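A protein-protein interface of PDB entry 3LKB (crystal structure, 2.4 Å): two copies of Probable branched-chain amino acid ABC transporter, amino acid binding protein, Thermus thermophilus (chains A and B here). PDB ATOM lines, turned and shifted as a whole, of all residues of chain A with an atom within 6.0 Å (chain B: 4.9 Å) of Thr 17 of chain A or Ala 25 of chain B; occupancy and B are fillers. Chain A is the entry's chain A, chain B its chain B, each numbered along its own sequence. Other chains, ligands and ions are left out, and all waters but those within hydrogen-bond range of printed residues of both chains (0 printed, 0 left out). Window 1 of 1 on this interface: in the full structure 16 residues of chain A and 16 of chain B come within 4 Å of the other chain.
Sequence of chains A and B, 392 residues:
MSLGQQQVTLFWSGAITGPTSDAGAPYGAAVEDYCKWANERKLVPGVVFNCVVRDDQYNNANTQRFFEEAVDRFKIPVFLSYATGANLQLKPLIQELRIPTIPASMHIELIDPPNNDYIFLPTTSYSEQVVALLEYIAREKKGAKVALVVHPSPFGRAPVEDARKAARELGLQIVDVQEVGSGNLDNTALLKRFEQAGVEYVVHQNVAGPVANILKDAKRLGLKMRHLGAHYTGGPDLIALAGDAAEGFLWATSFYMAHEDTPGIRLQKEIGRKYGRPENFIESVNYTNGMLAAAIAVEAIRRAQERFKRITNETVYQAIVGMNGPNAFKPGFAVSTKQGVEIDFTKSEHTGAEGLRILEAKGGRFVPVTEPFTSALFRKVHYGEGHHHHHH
OG1 of Thr 17 of chain A is in hydrogen-bond range of OD2 of Asp 55 of chain A (2.8 Å). The backbone NH (N) of Gln 57 of chain A sits at hydrogen-bond distance from the side-chain carboxylate (OD1) of Asp 55 of chain A, at 3.0 Å. The backbone NH of Ala 25 of chain B lies within hydrogen-bond range of the backbone carbonyl oxygen of Ala 15 of chain B (3.5 Å).
Ile 16 of chain B touches Thr 17 of chain A. Thr 17 of chain A touches Ala 25 of chain B (CG2 to CB, 3.9 Å). Thr 17 of chain A touches Phe 281 of chain B (OG1 to CZ, 3.7 Å). Gln 57 of chain A touches Phe 281 of chain B (NE2 to CE1, 3.6 Å).
Printed residues of chain B within 4 Å of Thr 17 of chain A: Ile 16, Ala 25 and Phe 281. Of the printed residues of chain B, Gln 57 of chain A touches Phe 281. Of the printed residues of chain A, Ile 16 of chain B touches Thr 17 (3.8 Å).
Printed residues of chain A that touch a printed residue of chain B: Thr 17 and Gln 57. Along chain A the printed residues that touch a printed residue of chain B span positions 17 to 57. Hydrophobic or aromatic side chains of chain B within 4 Å of the printed part of chain A: Ile 16, Ala 25 and Phe 281. Along chain B the printed residues that touch a printed residue of chain A span positions 16 to 281. Among the printed residues, 4 pairs touch across the chains. Among the printed residues, no Asp or Glu carboxylate lies within 4 Å of a Lys or Arg side-chain nitrogen of the other chain.
4 positions are printed for both chains.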
ATOM      1  N   GLY A  14       0.758  17.318  13.303  1.00  0.00           N
ATOM      2  CA  GLY A  14      -0.026  16.095  13.470  1.00  0.00           C
ATOM      3  C   GLY A  14      -0.284  15.445  12.127  1.00  0.00           C
ATOM      4  O   GLY A  14       0.296  15.840  11.098  1.00  0.00           O
ATOM      5  N   ALA A  15      -1.103  14.396  12.151  1.00  0.00           N
ATOM      6  CA  ALA A  15      -1.334  13.504  11.037  1.00  0.00           C
ATOM      7  C   ALA A  15      -2.526  13.943  10.172  1.00  0.00           C
ATOM      8  O   ALA A  15      -3.646  13.421  10.363  1.00  0.00           O
ATOM      9  CB  ALA A  15      -1.592  12.105  11.564  1.00  0.00           C
ATOM     10  N   ILE A  16      -2.278  14.870   9.235  1.00  0.00           N
ATOM     11  CA  ILE A  16      -3.253  15.263   8.220  1.00  0.00           C
ATOM     12  C   ILE A  16      -3.402  14.058   7.266  1.00  0.00           C
ATOM     13  O   ILE A  16      -4.498  13.790   6.728  1.00  0.00           O
ATOM     14  CB  ILE A  16      -2.795  16.571   7.477  1.00  0.00           C
ATOM     15  CG1 ILE A  16      -2.949  17.801   8.366  1.00  0.00           C
ATOM     16  CG2 ILE A  16      -3.692  16.894   6.325  1.00  0.00           C
ATOM     17  CD1 ILE A  16      -1.830  18.807   8.174  1.00  0.00           C
ATOM     18  N   THR A  17      -2.306  13.297   7.095  1.00  0.00           N
ATOM     19  CA  THR A  17      -2.371  12.052   6.354  1.00  0.00           C
ATOM     20  C   THR A  17      -1.630  11.013   7.121  1.00  0.00           C
ATOM     21  O   THR A  17      -1.069  11.334   8.163  1.00  0.00           O
ATOM     22  CB  THR A  17      -1.815  12.185   4.932  1.00  0.00           C
ATOM     23  OG1 THR A  17      -0.380  12.408   4.962  1.00  0.00           O
ATOM     24  CG2 THR A  17      -2.553  13.339   4.213  1.00  0.00           C
ATOM     25  N   GLY A  18      -1.650   9.761   6.636  1.00  0.00           N
ATOM     26  CA  GLY A  18      -0.999   8.654   7.321  1.00  0.00           C
ATOM     27  C   GLY A  18      -1.841   8.123   8.447  1.00  0.00           C
ATOM     28  O   GLY A  18      -3.021   8.439   8.541  1.00  0.00           O
ATOM     29  N   PRO A  19      -1.245   7.297   9.310  1.00  0.00           N
ATOM     30  CA  PRO A  19      -2.008   6.593  10.354  1.00  0.00           C
ATOM     31  C   PRO A  19      -2.777   7.564  11.244  1.00  0.00           C
ATOM     32  O   PRO A  19      -2.219   8.607  11.623  1.00  0.00           O
ATOM     33  CB  PRO A  19      -0.909   5.886  11.191  1.00  0.00           C
ATOM     34  CG  PRO A  19       0.305   5.802  10.281  1.00  0.00           C
ATOM     35  CD  PRO A  19       0.202   7.015   9.368  1.00  0.00           C
ATOM     36  N   SER A  21      -5.206   9.446  10.534  1.00  0.00           N
ATOM     37  CA  SER A  21      -5.637  10.646   9.827  1.00  0.00           C
ATOM     38  C   SER A  21      -7.171  10.852   9.744  1.00  0.00           C
ATOM     39  O   SER A  21      -7.650  11.954   9.517  1.00  0.00           O
ATOM     40  CB  SER A  21      -4.915  10.756   8.482  1.00  0.00           C
ATOM     41  OG  SER A  21      -5.288   9.713   7.615  1.00  0.00           O
ATOM     42  N   ALA A  25      -6.923  14.827  10.222  1.00  0.00           N
ATOM     43  CA  ALA A  25      -7.289  15.715   9.120  1.00  0.00           C
ATOM     44  C   ALA A  25      -8.281  16.837   9.557  1.00  0.00           C
ATOM     45  O   ALA A  25      -7.953  18.028   9.489  1.00  0.00           O
ATOM     46  CB  ALA A  25      -7.807  14.913   7.909  1.00  0.00           C
ATOM     47  N   ASP A  55       1.866  18.492   8.590  1.00  0.00           N
ATOM     48  CA  ASP A  55       1.547  17.119   8.534  1.00  0.00           C
ATOM     49  C   ASP A  55       2.799  16.307   8.835  1.00  0.00           C
ATOM     50  O   ASP A  55       3.670  16.204   7.981  1.00  0.00           O
ATOM     51  CB  ASP A  55       1.091  16.802   7.112  1.00  0.00           C
ATOM     52  CG  ASP A  55       0.706  15.320   6.923  1.00  0.00           C
ATOM     53  OD1 ASP A  55       0.426  14.583   7.904  1.00  0.00           O
ATOM     54  OD2 ASP A  55       0.680  14.893   5.760  1.00  0.00           O
ATOM     55  N   ASP A  56       2.870  15.714  10.035  1.00  0.00           N
ATOM     56  CA  ASP A  56       3.949  14.807  10.388  1.00  0.00           C
ATOM     57  C   ASP A  56       3.661  13.352  10.074  1.00  0.00           C
ATOM     58  O   ASP A  56       4.511  12.512  10.335  1.00  0.00           O
ATOM     59  CB  ASP A  56       4.310  14.922  11.874  1.00  0.00           C
ATOM     60  CG  ASP A  56       3.118  14.598  12.826  1.00  0.00           C
ATOM     61  OD1 ASP A  56       2.252  13.734  12.496  1.00  0.00           O
ATOM     62  OD2 ASP A  56       3.071  15.227  13.923  1.00  0.00           O
ATOM     63  N   GLN A  57       2.462  13.059   9.561  1.00  0.00           N
ATOM     64  CA  GLN A  57       2.020  11.691   9.226  1.00  0.00           C
ATOM     65  C   GLN A  57       2.223  10.648  10.338  1.00  0.00           C
ATOM     66  O   GLN A  57       2.424   9.463  10.065  1.00  0.00           O
ATOM     67  CB  GLN A  57       2.676  11.229   7.931  1.00  0.00           C
ATOM     68  CG  GLN A  57       2.327  12.174   6.766  1.00  0.00           C
ATOM     69  CD  GLN A  57       2.765  11.674   5.436  1.00  0.00           C
ATOM     70  OE1 GLN A  57       3.943  11.379   5.237  1.00  0.00           O
ATOM     71  NE2 GLN A  57       1.816  11.568   4.494  1.00  0.00           N
ATOM     72  N   TYR A  58       2.145  11.096  11.586  1.00  0.00           N
ATOM     73  CA  TYR A  58       2.262  10.201  12.730  1.00  0.00           C
ATOM     74  C   TYR A  58       3.672   9.666  12.852  1.00  0.00           C
ATOM     75  O   TYR A  58       3.860   8.616  13.408  1.00  0.00           O
ATOM     76  CB  TYR A  58       1.297   8.999  12.600  1.00  0.00           C
ATOM     77  CG  TYR A  58       0.675   8.590  13.910  1.00  0.00           C
ATOM     78  CD1 TYR A  58      -0.041   9.510  14.657  1.00  0.00           C
ATOM     79  CD2 TYR A  58       0.823   7.298  14.421  1.00  0.00           C
ATOM     80  CE1 TYR A  58      -0.597   9.163  15.858  1.00  0.00           C
ATOM     81  CE2 TYR A  58       0.261   6.939  15.652  1.00  0.00           C
ATOM     82  CZ  TYR A  58      -0.459   7.881  16.346  1.00  0.00           C
ATOM     83  OH  TYR A  58      -1.039   7.588  17.529  1.00  0.00           O
ATOM     84  N   ALA B  15      -6.451  17.953  -3.640  1.00  0.00           N
ATOM     85  CA  ALA B  15      -7.170  17.338  -2.532  1.00  0.00           C
ATOM     86  C   ALA B  15      -6.231  16.521  -1.671  1.00  0.00           C
ATOM     87  O   ALA B  15      -6.132  15.321  -1.847  1.00  0.00           O
ATOM     88  CB  ALA B  15      -8.305  16.434  -3.046  1.00  0.00           C
ATOM     89  N   ILE B  16      -5.512  17.167  -0.766  1.00  0.00           N
ATOM     90  CA  ILE B  16      -4.803  16.413   0.272  1.00  0.00           C
ATOM     91  C   ILE B  16      -5.803  15.674   1.163  1.00  0.00           C
ATOM     92  O   ILE B  16      -5.541  14.521   1.545  1.00  0.00           O
ATOM     93  CB  ILE B  16      -3.832  17.298   1.095  1.00  0.00           C
ATOM     94  CG1 ILE B  16      -2.725  17.800   0.180  1.00  0.00           C
ATOM     95  CG2 ILE B  16      -3.168  16.507   2.269  1.00  0.00           C
ATOM     96  CD1 ILE B  16      -1.896  18.927   0.887  1.00  0.00           C
ATOM     97  N   SER B  21      -9.019  12.372  -2.342  1.00  0.00           N
ATOM     98  CA  SER B  21      -7.748  12.406  -1.575  1.00  0.00           C
ATOM     99  C   SER B  21      -6.963  11.098  -1.489  1.00  0.00           C
ATOM    100  O   SER B  21      -5.769  11.111  -1.162  1.00  0.00           O
ATOM    101  CB  SER B  21      -7.963  12.933  -0.160  1.00  0.00           C
ATOM    102  OG  SER B  21      -8.929  12.139   0.553  1.00  0.00           O
ATOM    103  N   ASP B  22      -7.598   9.961  -1.774  1.00  0.00           N
ATOM    104  CA  ASP B  22      -6.826   8.689  -1.847  1.00  0.00           C
ATOM    105  C   ASP B  22      -5.651   8.882  -2.853  1.00  0.00           C
ATOM    106  O   ASP B  22      -4.555   8.285  -2.715  1.00  0.00           O
ATOM    107  CB  ASP B  22      -7.726   7.533  -2.270  1.00  0.00           C
ATOM    108  CG  ASP B  22      -8.564   6.931  -1.083  1.00  0.00           C
ATOM    109  OD1 ASP B  22      -8.119   7.009   0.086  1.00  0.00           O
ATOM    110  OD2 ASP B  22      -9.678   6.367  -1.352  1.00  0.00           O
ATOM    111  N   ALA B  23      -5.910   9.742  -3.841  1.00  0.00           N
ATOM    112  CA  ALA B  23      -4.964  10.052  -4.873  1.00  0.00           C
ATOM    113  C   ALA B  23      -4.224  11.330  -4.542  1.00  0.00           C
ATOM    114  O   ALA B  23      -3.031  11.386  -4.737  1.00  0.00           O
ATOM    115  CB  ALA B  23      -5.684  10.207  -6.278  1.00  0.00           C
ATOM    116  N   GLY B  24      -4.928  12.362  -4.075  1.00  0.00           N
ATOM    117  CA  GLY B  24      -4.337  13.700  -4.015  1.00  0.00           C
ATOM    118  C   GLY B  24      -3.284  13.858  -2.941  1.00  0.00           C
ATOM    119  O   GLY B  24      -2.321  14.629  -3.086  1.00  0.00           O
ATOM    120  N   ALA B  25      -3.457  13.106  -1.858  1.00  0.00           N
ATOM    121  CA  ALA B  25      -2.546  13.134  -0.720  1.00  0.00           C
ATOM    122  C   ALA B  25      -1.133  12.652  -1.128  1.00  0.00           C
ATOM    123  O   ALA B  25      -0.186  13.399  -0.959  1.00  0.00           O
ATOM    124  CB  ALA B  25      -3.134  12.321   0.485  1.00  0.00           C
ATOM    125  N   PRO B  26      -0.994  11.428  -1.695  1.00  0.00           N
ATOM    126  CA  PRO B  26       0.344  10.969  -2.166  1.00  0.00           C
ATOM    127  C   PRO B  26       0.898  11.830  -3.303  1.00  0.00           C
ATOM    128  O   PRO B  26       2.100  12.011  -3.423  1.00  0.00           O
ATOM    129  CB  PRO B  26       0.097   9.523  -2.664  1.00  0.00           C
ATOM    130  CG  PRO B  26      -1.374   9.265  -2.535  1.00  0.00           C
ATOM    131  CD  PRO B  26      -2.012  10.352  -1.724  1.00  0.00           C
ATOM    132  N   TYR B  27       0.009  12.349  -4.134  1.00  0.00           N
ATOM    133  CA  TYR B  27       0.387  13.228  -5.229  1.00  0.00           C
ATOM    134  C   TYR B  27       1.004  14.509  -4.670  1.00  0.00           C
ATOM    135  O   TYR B  27       2.088  14.889  -5.076  1.00  0.00           O
ATOM    136  CB  TYR B  27      -0.854  13.579  -6.044  1.00  0.00           C
ATOM    137  CG  TYR B  27      -0.525  14.178  -7.382  1.00  0.00           C
ATOM    138  CD1 TYR B  27      -0.627  13.423  -8.569  1.00  0.00           C
ATOM    139  CD2 TYR B  27      -0.132  15.512  -7.489  1.00  0.00           C
ATOM    140  CE1 TYR B  27      -0.325  14.003  -9.809  1.00  0.00           C
ATOM    141  CE2 TYR B  27       0.144  16.089  -8.699  1.00  0.00           C
ATOM    142  CZ  TYR B  27       0.058  15.343  -9.864  1.00  0.00           C
ATOM    143  OH  TYR B  27       0.334  15.978 -11.093  1.00  0.00           O
ATOM    144  N   GLY B  28       0.300  15.157  -3.740  1.00  0.00           N
ATOM    145  CA  GLY B  28       0.788  16.396  -3.100  1.00  0.00           C
ATOM    146  C   GLY B  28       2.058  16.149  -2.273  1.00  0.00           C
ATOM    147  O   GLY B  28       2.977  16.953  -2.265  1.00  0.00           O
ATOM    148  N   ALA B  29       2.097  15.011  -1.590  1.00  0.00           N
ATOM    149  CA  ALA B  29       3.294  14.595  -0.838  1.00  0.00           C
ATOM    150  C   ALA B  29       4.516  14.512  -1.750  1.00  0.00           C
ATOM    151  O   ALA B  29       5.582  14.994  -1.355  1.00  0.00           O
ATOM    152  CB  ALA B  29       3.052  13.308  -0.083  1.00  0.00           C
ATOM    153  N   PHE B 281       2.478   5.385   1.112  1.00  0.00           N
ATOM    154  CA  PHE B 281       2.694   6.530   0.240  1.00  0.00           C
ATOM    155  C   PHE B 281       3.853   6.257  -0.714  1.00  0.00           C
ATOM    156  O   PHE B 281       3.841   6.680  -1.886  1.00  0.00           O
ATOM    157  CB  PHE B 281       2.973   7.817   1.048  1.00  0.00           C
ATOM    158  CG  PHE B 281       1.714   8.544   1.510  1.00  0.00           C
ATOM    159  CD1 PHE B 281       1.427   9.840   1.057  1.00  0.00           C
ATOM    160  CD2 PHE B 281       0.837   7.946   2.393  1.00  0.00           C
ATOM    161  CE1 PHE B 281       0.260  10.489   1.468  1.00  0.00           C
ATOM    162  CE2 PHE B 281      -0.339   8.583   2.786  1.00  0.00           C
ATOM    163  CZ  PHE B 281      -0.629   9.847   2.319  1.00  0.00           C
